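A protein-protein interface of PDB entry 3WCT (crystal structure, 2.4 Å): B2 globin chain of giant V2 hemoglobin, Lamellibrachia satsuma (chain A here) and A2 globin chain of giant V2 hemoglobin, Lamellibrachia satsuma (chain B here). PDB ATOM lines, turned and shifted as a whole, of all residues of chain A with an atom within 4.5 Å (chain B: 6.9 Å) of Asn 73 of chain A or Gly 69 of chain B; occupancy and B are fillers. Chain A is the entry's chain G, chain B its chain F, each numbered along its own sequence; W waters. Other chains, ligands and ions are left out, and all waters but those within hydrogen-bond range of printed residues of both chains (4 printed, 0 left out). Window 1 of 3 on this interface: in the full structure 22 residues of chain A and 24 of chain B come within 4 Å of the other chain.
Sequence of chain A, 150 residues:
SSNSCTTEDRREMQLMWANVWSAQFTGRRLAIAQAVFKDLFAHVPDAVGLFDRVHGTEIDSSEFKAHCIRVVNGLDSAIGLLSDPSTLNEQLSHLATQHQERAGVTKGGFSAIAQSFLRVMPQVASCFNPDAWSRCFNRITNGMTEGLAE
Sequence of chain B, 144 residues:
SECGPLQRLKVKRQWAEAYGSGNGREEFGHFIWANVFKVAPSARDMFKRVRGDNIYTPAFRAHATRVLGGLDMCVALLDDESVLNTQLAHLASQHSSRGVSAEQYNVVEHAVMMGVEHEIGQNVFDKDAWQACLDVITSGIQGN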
ATOM      1  N   ILE A  69      23.207 -20.786 -13.892  1.00  0.00           N
ATOM      2  CA  ILE A  69      23.966 -21.814 -13.228  1.00  0.00           C
ATOM      3  C   ILE A  69      24.446 -21.307 -11.868  1.00  0.00           C
ATOM      4  O   ILE A  69      24.406 -22.043 -10.881  1.00  0.00           O
ATOM      5  CB  ILE A  69      25.146 -22.257 -14.123  1.00  0.00           C
ATOM      6  CG1 ILE A  69      24.590 -23.097 -15.272  1.00  0.00           C
ATOM      7  CG2 ILE A  69      26.182 -23.030 -13.321  1.00  0.00           C
ATOM      8  CD1 ILE A  69      25.628 -23.538 -16.286  1.00  0.00           C
ATOM      9  N   ARG A  70      24.859 -20.041 -11.812  1.00  0.00           N
ATOM     10  CA  ARG A  70      25.339 -19.449 -10.562  1.00  0.00           C
ATOM     11  C   ARG A  70      24.212 -19.305  -9.552  1.00  0.00           C
ATOM     12  O   ARG A  70      24.444 -19.393  -8.348  1.00  0.00           O
ATOM     13  CB  ARG A  70      25.986 -18.075 -10.801  1.00  0.00           C
ATOM     14  CG  ARG A  70      27.330 -18.100 -11.544  1.00  0.00           C
ATOM     15  CD  ARG A  70      28.058 -16.709 -11.506  1.00  0.00           C
ATOM     16  NE  ARG A  70      27.445 -15.649 -12.317  1.00  0.00           N
ATOM     17  CZ  ARG A  70      27.623 -15.479 -13.630  1.00  0.00           C
ATOM     18  NH1 ARG A  70      28.401 -16.297 -14.329  1.00  0.00           N
ATOM     19  NH2 ARG A  70      27.036 -14.462 -14.251  1.00  0.00           N
ATOM     20  N   VAL A  71      22.994 -19.085 -10.041  1.00  0.00           N
ATOM     21  CA  VAL A  71      21.827 -18.936  -9.174  1.00  0.00           C
ATOM     22  C   VAL A  71      21.404 -20.264  -8.544  1.00  0.00           C
ATOM     23  O   VAL A  71      21.152 -20.330  -7.343  1.00  0.00           O
ATOM     24  CB  VAL A  71      20.611 -18.352  -9.946  1.00  0.00           C
ATOM     25  CG1 VAL A  71      19.354 -18.416  -9.078  1.00  0.00           C
ATOM     26  CG2 VAL A  71      20.890 -16.894 -10.325  1.00  0.00           C
ATOM     27  N   VAL A  72      21.307 -21.319  -9.348  1.00  0.00           N
ATOM     28  CA  VAL A  72      20.903 -22.606  -8.805  1.00  0.00           C
ATOM     29  C   VAL A  72      22.017 -23.171  -7.919  1.00  0.00           C
ATOM     30  O   VAL A  72      21.753 -23.927  -7.002  1.00  0.00           O
ATOM     31  CB  VAL A  72      20.506 -23.600  -9.935  1.00  0.00           C
ATOM     32  CG1 VAL A  72      19.130 -23.243 -10.464  1.00  0.00           C
ATOM     33  CG2 VAL A  72      21.492 -23.545 -11.057  1.00  0.00           C
ATOM     34  N   ASN A  73      23.261 -22.786  -8.195  1.00  0.00           N
ATOM     35  CA  ASN A  73      24.400 -23.212  -7.385  1.00  0.00           C
ATOM     36  C   ASN A  73      24.279 -22.542  -6.013  1.00  0.00           C
ATOM     37  O   ASN A  73      24.614 -23.130  -4.981  1.00  0.00           O
ATOM     38  CB  ASN A  73      25.716 -22.789  -8.039  1.00  0.00           C
ATOM     39  CG  ASN A  73      26.924 -23.068  -7.155  1.00  0.00           C
ATOM     40  OD1 ASN A  73      27.250 -24.223  -6.866  1.00  0.00           O
ATOM     41  ND2 ASN A  73      27.590 -22.002  -6.709  1.00  0.00           N
ATOM     42  N   GLY A  74      23.787 -21.304  -6.017  1.00  0.00           N
ATOM     43  CA  GLY A  74      23.615 -20.559  -4.780  1.00  0.00           C
ATOM     44  C   GLY A  74      22.495 -21.145  -3.953  1.00  0.00           C
ATOM     45  O   GLY A  74      22.613 -21.274  -2.724  1.00  0.00           O
ATOM     46  N   LEU A  75      21.400 -21.497  -4.630  1.00  0.00           N
ATOM     47  CA  LEU A  75      20.250 -22.084  -3.963  1.00  0.00           C
ATOM     48  C   LEU A  75      20.632 -23.486  -3.483  1.00  0.00           C
ATOM     49  O   LEU A  75      20.248 -23.909  -2.393  1.00  0.00           O
ATOM     50  CB  LEU A  75      19.058 -22.168  -4.926  1.00  0.00           C
ATOM     51  CG  LEU A  75      17.801 -22.831  -4.369  1.00  0.00           C
ATOM     52  CD1 LEU A  75      17.397 -22.127  -3.088  1.00  0.00           C
ATOM     53  CD2 LEU A  75      16.663 -22.804  -5.429  1.00  0.00           C
ATOM     54  N   ASP A  76      21.400 -24.194  -4.302  1.00  0.00           N
ATOM     55  CA  ASP A  76      21.827 -25.537  -3.960  1.00  0.00           C
ATOM     56  C   ASP A  76      22.644 -25.547  -2.673  1.00  0.00           C
ATOM     57  O   ASP A  76      22.431 -26.385  -1.803  1.00  0.00           O
ATOM     58  CB  ASP A  76      22.644 -26.143  -5.102  1.00  0.00           C
ATOM     59  CG  ASP A  76      23.196 -27.503  -4.753  1.00  0.00           C
ATOM     60  OD1 ASP A  76      24.383 -27.580  -4.387  1.00  0.00           O
ATOM     61  OD2 ASP A  76      22.435 -28.486  -4.828  1.00  0.00           O
ATOM     62  N   SER A  77      23.567 -24.597  -2.558  1.00  0.00           N
ATOM     63  CA  SER A  77      24.422 -24.489  -1.389  1.00  0.00           C
ATOM     64  C   SER A  77      23.575 -24.172  -0.162  1.00  0.00           C
ATOM     65  O   SER A  77      23.861 -24.635   0.942  1.00  0.00           O
ATOM     66  CB  SER A  77      25.458 -23.382  -1.588  1.00  0.00           C
ATOM     67  OG  SER A  77      24.866 -22.085  -1.471  1.00  0.00           O
ATOM     68  N   TRP B  15      33.838 -36.573  -9.684  1.00  0.00           N
ATOM     69  CA  TRP B  15      33.502 -35.372  -8.921  1.00  0.00           C
ATOM     70  C   TRP B  15      32.139 -35.528  -8.233  1.00  0.00           C
ATOM     71  O   TRP B  15      31.977 -35.175  -7.058  1.00  0.00           O
ATOM     72  CB  TRP B  15      33.485 -34.130  -9.820  1.00  0.00           C
ATOM     73  CG  TRP B  15      32.858 -32.955  -9.146  1.00  0.00           C
ATOM     74  CD1 TRP B  15      31.590 -32.501  -9.325  1.00  0.00           C
ATOM     75  CD2 TRP B  15      33.434 -32.149  -8.109  1.00  0.00           C
ATOM     76  NE1 TRP B  15      31.333 -31.463  -8.460  1.00  0.00           N
ATOM     77  CE2 TRP B  15      32.448 -31.225  -7.703  1.00  0.00           C
ATOM     78  CE3 TRP B  15      34.686 -32.121  -7.483  1.00  0.00           C
ATOM     79  CZ2 TRP B  15      32.668 -30.276  -6.693  1.00  0.00           C
ATOM     80  CZ3 TRP B  15      34.910 -31.175  -6.470  1.00  0.00           C
ATOM     81  CH2 TRP B  15      33.901 -30.266  -6.089  1.00  0.00           C
ATOM     82  N   TYR B  19      31.880 -35.157  -4.372  1.00  0.00           N
ATOM     83  CA  TYR B  19      31.037 -34.052  -3.949  1.00  0.00           C
ATOM     84  C   TYR B  19      29.729 -34.553  -3.346  1.00  0.00           C
ATOM     85  O   TYR B  19      29.234 -33.987  -2.374  1.00  0.00           O
ATOM     86  CB  TYR B  19      30.776 -33.122  -5.132  1.00  0.00           C
ATOM     87  CG  TYR B  19      30.243 -31.760  -4.760  1.00  0.00           C
ATOM     88  CD1 TYR B  19      30.768 -31.048  -3.675  1.00  0.00           C
ATOM     89  CD2 TYR B  19      29.259 -31.150  -5.538  1.00  0.00           C
ATOM     90  CE1 TYR B  19      30.325 -29.758  -3.382  1.00  0.00           C
ATOM     91  CE2 TYR B  19      28.817 -29.872  -5.258  1.00  0.00           C
ATOM     92  CZ  TYR B  19      29.353 -29.180  -4.183  1.00  0.00           C
ATOM     93  OH  TYR B  19      28.922 -27.901  -3.947  1.00  0.00           O
ATOM     94  N   ARG B  25      29.590 -33.045   2.128  1.00  0.00           N
ATOM     95  CA  ARG B  25      30.358 -31.899   1.640  1.00  0.00           C
ATOM     96  C   ARG B  25      31.179 -31.155   2.699  1.00  0.00           C
ATOM     97  O   ARG B  25      32.256 -30.626   2.388  1.00  0.00           O
ATOM     98  CB  ARG B  25      29.434 -30.903   0.931  1.00  0.00           C
ATOM     99  CG  ARG B  25      28.807 -31.430  -0.352  1.00  0.00           C
ATOM    100  CD  ARG B  25      27.915 -30.377  -1.009  1.00  0.00           C
ATOM    101  NE  ARG B  25      27.229 -30.920  -2.172  1.00  0.00           N
ATOM    102  CZ  ARG B  25      26.299 -30.271  -2.868  1.00  0.00           C
ATOM    103  NH1 ARG B  25      25.936 -29.042  -2.518  1.00  0.00           N
ATOM    104  NH2 ARG B  25      25.727 -30.855  -3.914  1.00  0.00           N
ATOM    105  N   HIS B  63      32.916 -20.173   3.192  1.00  0.00           N
ATOM    106  CA  HIS B  63      33.833 -19.892   2.096  1.00  0.00           C
ATOM    107  C   HIS B  63      34.139 -21.195   1.338  1.00  0.00           C
ATOM    108  O   HIS B  63      34.147 -21.218   0.107  1.00  0.00           O
ATOM    109  CB  HIS B  63      35.141 -19.285   2.625  1.00  0.00           C
ATOM    110  CG  HIS B  63      36.229 -19.222   1.598  1.00  0.00           C
ATOM    111  ND1 HIS B  63      36.176 -18.384   0.504  1.00  0.00           N
ATOM    112  CD2 HIS B  63      37.362 -19.952   1.453  1.00  0.00           C
ATOM    113  CE1 HIS B  63      37.221 -18.603  -0.270  1.00  0.00           C
ATOM    114  NE2 HIS B  63      37.958 -19.552   0.282  1.00  0.00           N
ATOM    115  N   ALA B  64      34.405 -22.269   2.080  1.00  0.00           N
ATOM    116  CA  ALA B  64      34.703 -23.574   1.480  1.00  0.00           C
ATOM    117  C   ALA B  64      33.514 -23.995   0.615  1.00  0.00           C
ATOM    118  O   ALA B  64      33.680 -24.505  -0.494  1.00  0.00           O
ATOM    119  CB  ALA B  64      34.945 -24.607   2.574  1.00  0.00           C
ATOM    120  N   THR B  65      32.312 -23.771   1.133  1.00  0.00           N
ATOM    121  CA  THR B  65      31.105 -24.100   0.403  1.00  0.00           C
ATOM    122  C   THR B  65      31.122 -23.378  -0.924  1.00  0.00           C
ATOM    123  O   THR B  65      30.803 -23.964  -1.953  1.00  0.00           O
ATOM    124  CB  THR B  65      29.850 -23.644   1.130  1.00  0.00           C
ATOM    125  OG1 THR B  65      29.772 -24.279   2.407  1.00  0.00           O
ATOM    126  CG2 THR B  65      28.615 -24.012   0.315  1.00  0.00           C
ATOM    127  N   ARG B  66      31.494 -22.100  -0.899  1.00  0.00           N
ATOM    128  CA  ARG B  66      31.531 -21.307  -2.128  1.00  0.00           C
ATOM    129  C   ARG B  66      32.577 -21.830  -3.113  1.00  0.00           C
ATOM    130  O   ARG B  66      32.301 -21.951  -4.311  1.00  0.00           O
ATOM    131  CB  ARG B  66      31.796 -19.818  -1.820  1.00  0.00           C
ATOM    132  CG  ARG B  66      30.619 -19.073  -1.158  1.00  0.00           C
ATOM    133  CD  ARG B  66      30.872 -17.539  -1.046  1.00  0.00           C
ATOM    134  NE  ARG B  66      31.828 -17.178   0.002  1.00  0.00           N
ATOM    135  CZ  ARG B  66      31.534 -17.109   1.299  1.00  0.00           C
ATOM    136  NH1 ARG B  66      32.464 -16.773   2.186  1.00  0.00           N
ATOM    137  NH2 ARG B  66      30.301 -17.366   1.711  1.00  0.00           N
ATOM    138  N   VAL B  67      33.774 -22.148  -2.621  1.00  0.00           N
ATOM    139  CA  VAL B  67      34.824 -22.644  -3.509  1.00  0.00           C
ATOM    140  C   VAL B  67      34.402 -23.952  -4.191  1.00  0.00           C
ATOM    141  O   VAL B  67      34.535 -24.105  -5.413  1.00  0.00           O
ATOM    142  CB  VAL B  67      36.138 -22.893  -2.752  1.00  0.00           C
ATOM    143  CG1 VAL B  67      37.217 -23.382  -3.725  1.00  0.00           C
ATOM    144  CG2 VAL B  67      36.592 -21.626  -2.068  1.00  0.00           C
ATOM    145  N   LEU B  68      33.893 -24.894  -3.406  1.00  0.00           N
ATOM    146  CA  LEU B  68      33.472 -26.167  -3.970  1.00  0.00           C
ATOM    147  C   LEU B  68      32.316 -25.942  -4.951  1.00  0.00           C
ATOM    148  O   LEU B  68      32.230 -26.607  -5.986  1.00  0.00           O
ATOM    149  CB  LEU B  68      33.067 -27.144  -2.859  1.00  0.00           C
ATOM    150  CG  LEU B  68      34.187 -27.493  -1.869  1.00  0.00           C
ATOM    151  CD1 LEU B  68      33.892 -28.834  -1.152  1.00  0.00           C
ATOM    152  CD2 LEU B  68      35.510 -27.579  -2.608  1.00  0.00           C
ATOM    153  N   GLY B  69      31.441 -24.993  -4.630  1.00  0.00           N
ATOM    154  CA  GLY B  69      30.329 -24.704  -5.516  1.00  0.00           C
ATOM    155  C   GLY B  69      30.894 -24.195  -6.837  1.00  0.00           C
ATOM    156  O   GLY B  69      30.369 -24.504  -7.912  1.00  0.00           O
ATOM    157  N   GLY B  70      31.977 -23.423  -6.750  1.00  0.00           N
ATOM    158  CA  GLY B  70      32.615 -22.896  -7.940  1.00  0.00           C
ATOM    159  C   GLY B  70      33.165 -24.036  -8.775  1.00  0.00           C
ATOM    160  O   GLY B  70      32.966 -24.101  -9.988  1.00  0.00           O
ATOM    161  N   LEU B  71      33.864 -24.950  -8.124  1.00  0.00           N
ATOM    162  CA  LEU B  71      34.424 -26.098  -8.821  1.00  0.00           C
ATOM    163  C   LEU B  71      33.322 -26.894  -9.494  1.00  0.00           C
ATOM    164  O   LEU B  71      33.482 -27.366 -10.615  1.00  0.00           O
ATOM    165  CB  LEU B  71      35.154 -27.020  -7.841  1.00  0.00           C
ATOM    166  CG  LEU B  71      36.587 -26.628  -7.540  1.00  0.00           C
ATOM    167  CD1 LEU B  71      37.174 -27.547  -6.472  1.00  0.00           C
ATOM    168  CD2 LEU B  71      37.374 -26.720  -8.834  1.00  0.00           C
ATOM    169  N   ASP B  72      32.200 -27.037  -8.794  1.00  0.00           N
ATOM    170  CA  ASP B  72      31.093 -27.818  -9.309  1.00  0.00           C
ATOM    171  C   ASP B  72      30.479 -27.242 -10.573  1.00  0.00           C
ATOM    172  O   ASP B  72      30.057 -27.988 -11.469  1.00  0.00           O
ATOM    173  CB  ASP B  72      30.018 -27.993  -8.233  1.00  0.00           C
ATOM    174  CG  ASP B  72      28.889 -28.886  -8.690  1.00  0.00           C
ATOM    175  OD1 ASP B  72      27.837 -28.345  -9.080  1.00  0.00           O
ATOM    176  OD2 ASP B  72      29.068 -30.128  -8.674  1.00  0.00           O
ATOM    177  N   MET B  73      30.426 -25.919 -10.657  1.00  0.00           N
ATOM    178  CA  MET B  73      29.858 -25.298 -11.841  1.00  0.00           C
ATOM    179  C   MET B  73      30.784 -25.582 -13.018  1.00  0.00           C
ATOM    180  O   MET B  73      30.327 -25.929 -14.110  1.00  0.00           O
ATOM    181  CB  MET B  73      29.681 -23.793 -11.623  1.00  0.00           C
ATOM    182  CG  MET B  73      28.644 -23.433 -10.551  1.00  0.00           C
ATOM    183  SD  MET B  73      28.253 -21.664 -10.446  1.00  0.00           S
ATOM    184  CE  MET B  73      29.568 -21.089  -9.360  1.00  0.00           C
ATOM    185  N   CYS B  74      32.086 -25.480 -12.780  1.00  0.00           N
ATOM    186  CA  CYS B  74      33.073 -25.723 -13.823  1.00  0.00           C
ATOM    187  C   CYS B  74      33.062 -27.169 -14.280  1.00  0.00           C
ATOM    188  O   CYS B  74      33.125 -27.455 -15.471  1.00  0.00           O
ATOM    189  CB  CYS B  74      34.478 -25.364 -13.328  1.00  0.00           C
ATOM    190  SG  CYS B  74      34.667 -23.634 -12.832  1.00  0.00           S
ATOM    191  N   GLN B  87      31.774 -18.786 -17.446  1.00  0.00           N
ATOM    192  CA  GLN B  87      31.808 -18.919 -15.994  1.00  0.00           C
ATOM    193  C   GLN B  87      33.242 -18.833 -15.488  1.00  0.00           C
ATOM    194  O   GLN B  87      33.486 -18.356 -14.380  1.00  0.00           O
ATOM    195  CB  GLN B  87      31.174 -20.240 -15.549  1.00  0.00           C
ATOM    196  CG  GLN B  87      31.264 -20.505 -14.045  1.00  0.00           C
ATOM    197  CD  GLN B  87      30.718 -19.363 -13.189  1.00  0.00           C
ATOM    198  OE1 GLN B  87      29.770 -18.680 -13.571  1.00  0.00           O
ATOM    199  NE2 GLN B  87      31.300 -19.180 -12.012  1.00  0.00           N
HETATM  200  O   HOH W   1      26.632 -25.959  -8.551  1.00  0.00           O
HETATM  201  O   HOH W   2      29.785 -20.575  -4.942  1.00  0.00           O
HETATM  202  O   HOH W   3      22.503 -31.129  -4.074  1.00  0.00           O
HETATM  203  O   HOH W   4      26.755 -26.957  -5.485  1.00  0.00           O
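The side-chain carboxylate of Asp 76 of chain A is in salt-bridge range of the guanidinium group of Arg 25 of chain B (2.8 Å).
The backbone carbonyl oxygen of Gly 69 of chain B lies close to the side-chain amide oxygen of Asn 73 of chain A, at 3.3 Å.
NH1 of Arg 70 of chain A sits at hydrogen-bond distance from OE1 of Gln 87 of chain B, at 2.9 Å.
The side-chain hydroxyl of Ser 77 of chain A is in hydrogen-bond range of the backbone carbonyl oxygen of Gly 74 of chain A, at 2.7 Å.
CG2 of Ile 69 of chain A touches CG of Met 73 of chain B, at 3.7 Å.
Arg 70 of chain A touches Met 73 of chain B (CA to SD, 3.7 Å).
CE of Met 73 of chain B touches ND2 of Asn 73 of chain A, at 3.4 Å.
Thr 65 of chain B touches Ser 77 of chain A (CG2 to CB, 3.7 Å).
Asn 73 of chain A touches just these residues of chain B: Gly 69 and Met 73.
Of the printed residues of chain B, Asp 76 of chain A touches Arg 25.
Of the printed residues of chain A, Gln 87 of chain B touches Arg 70 (2.9 Å).
Tyr 19 of chain B touches none of the printed residues of chain A.
The nearest printed residue of chain B that does not touch Ile 69 of chain A is Gln 87 of chain B (5.6 Å).
Hydrophobic or aromatic side chains of chain B that line the printed part of chain A: Met 73.
Of the 9 printed residues of chain A, 5 touch a printed residue of chain B.
Among the printed residues, 7 pairs touch across the chains.
Among the printed residues, Asp or Glu carboxylates within 4 Å of a Lys or Arg side-chain nitrogen of the other chain: Asp 76 of chain A with Arg 25 of chain B.
Water W1 bridges the side-chain amide oxygen (OD1) of Asn 73 of chain A (2.5 Å) and the side-chain carboxylate (OD1) of Asp 72 of chain B (2.7 Å).
Water W4 lies within hydrogen-bond range of the side-chain carboxylate (OD1) of Asp 76 of chain A, the side-chain hydroxyl (OH) of Tyr 19 of chain B and the side-chain amide oxygen (OD1) of Asn 73 of chain A.
Water W3 lies within hydrogen-bond range of the side-chain carboxylate of Asp 76 of chain A (2.7 Å) and the guanidinium group of Arg 25 of chain B (3.2 Å).
Water W2 bridges O of Arg 66 of chain B (2.9 Å) and ND2 of Asn 73 of chain A (3.2 Å).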
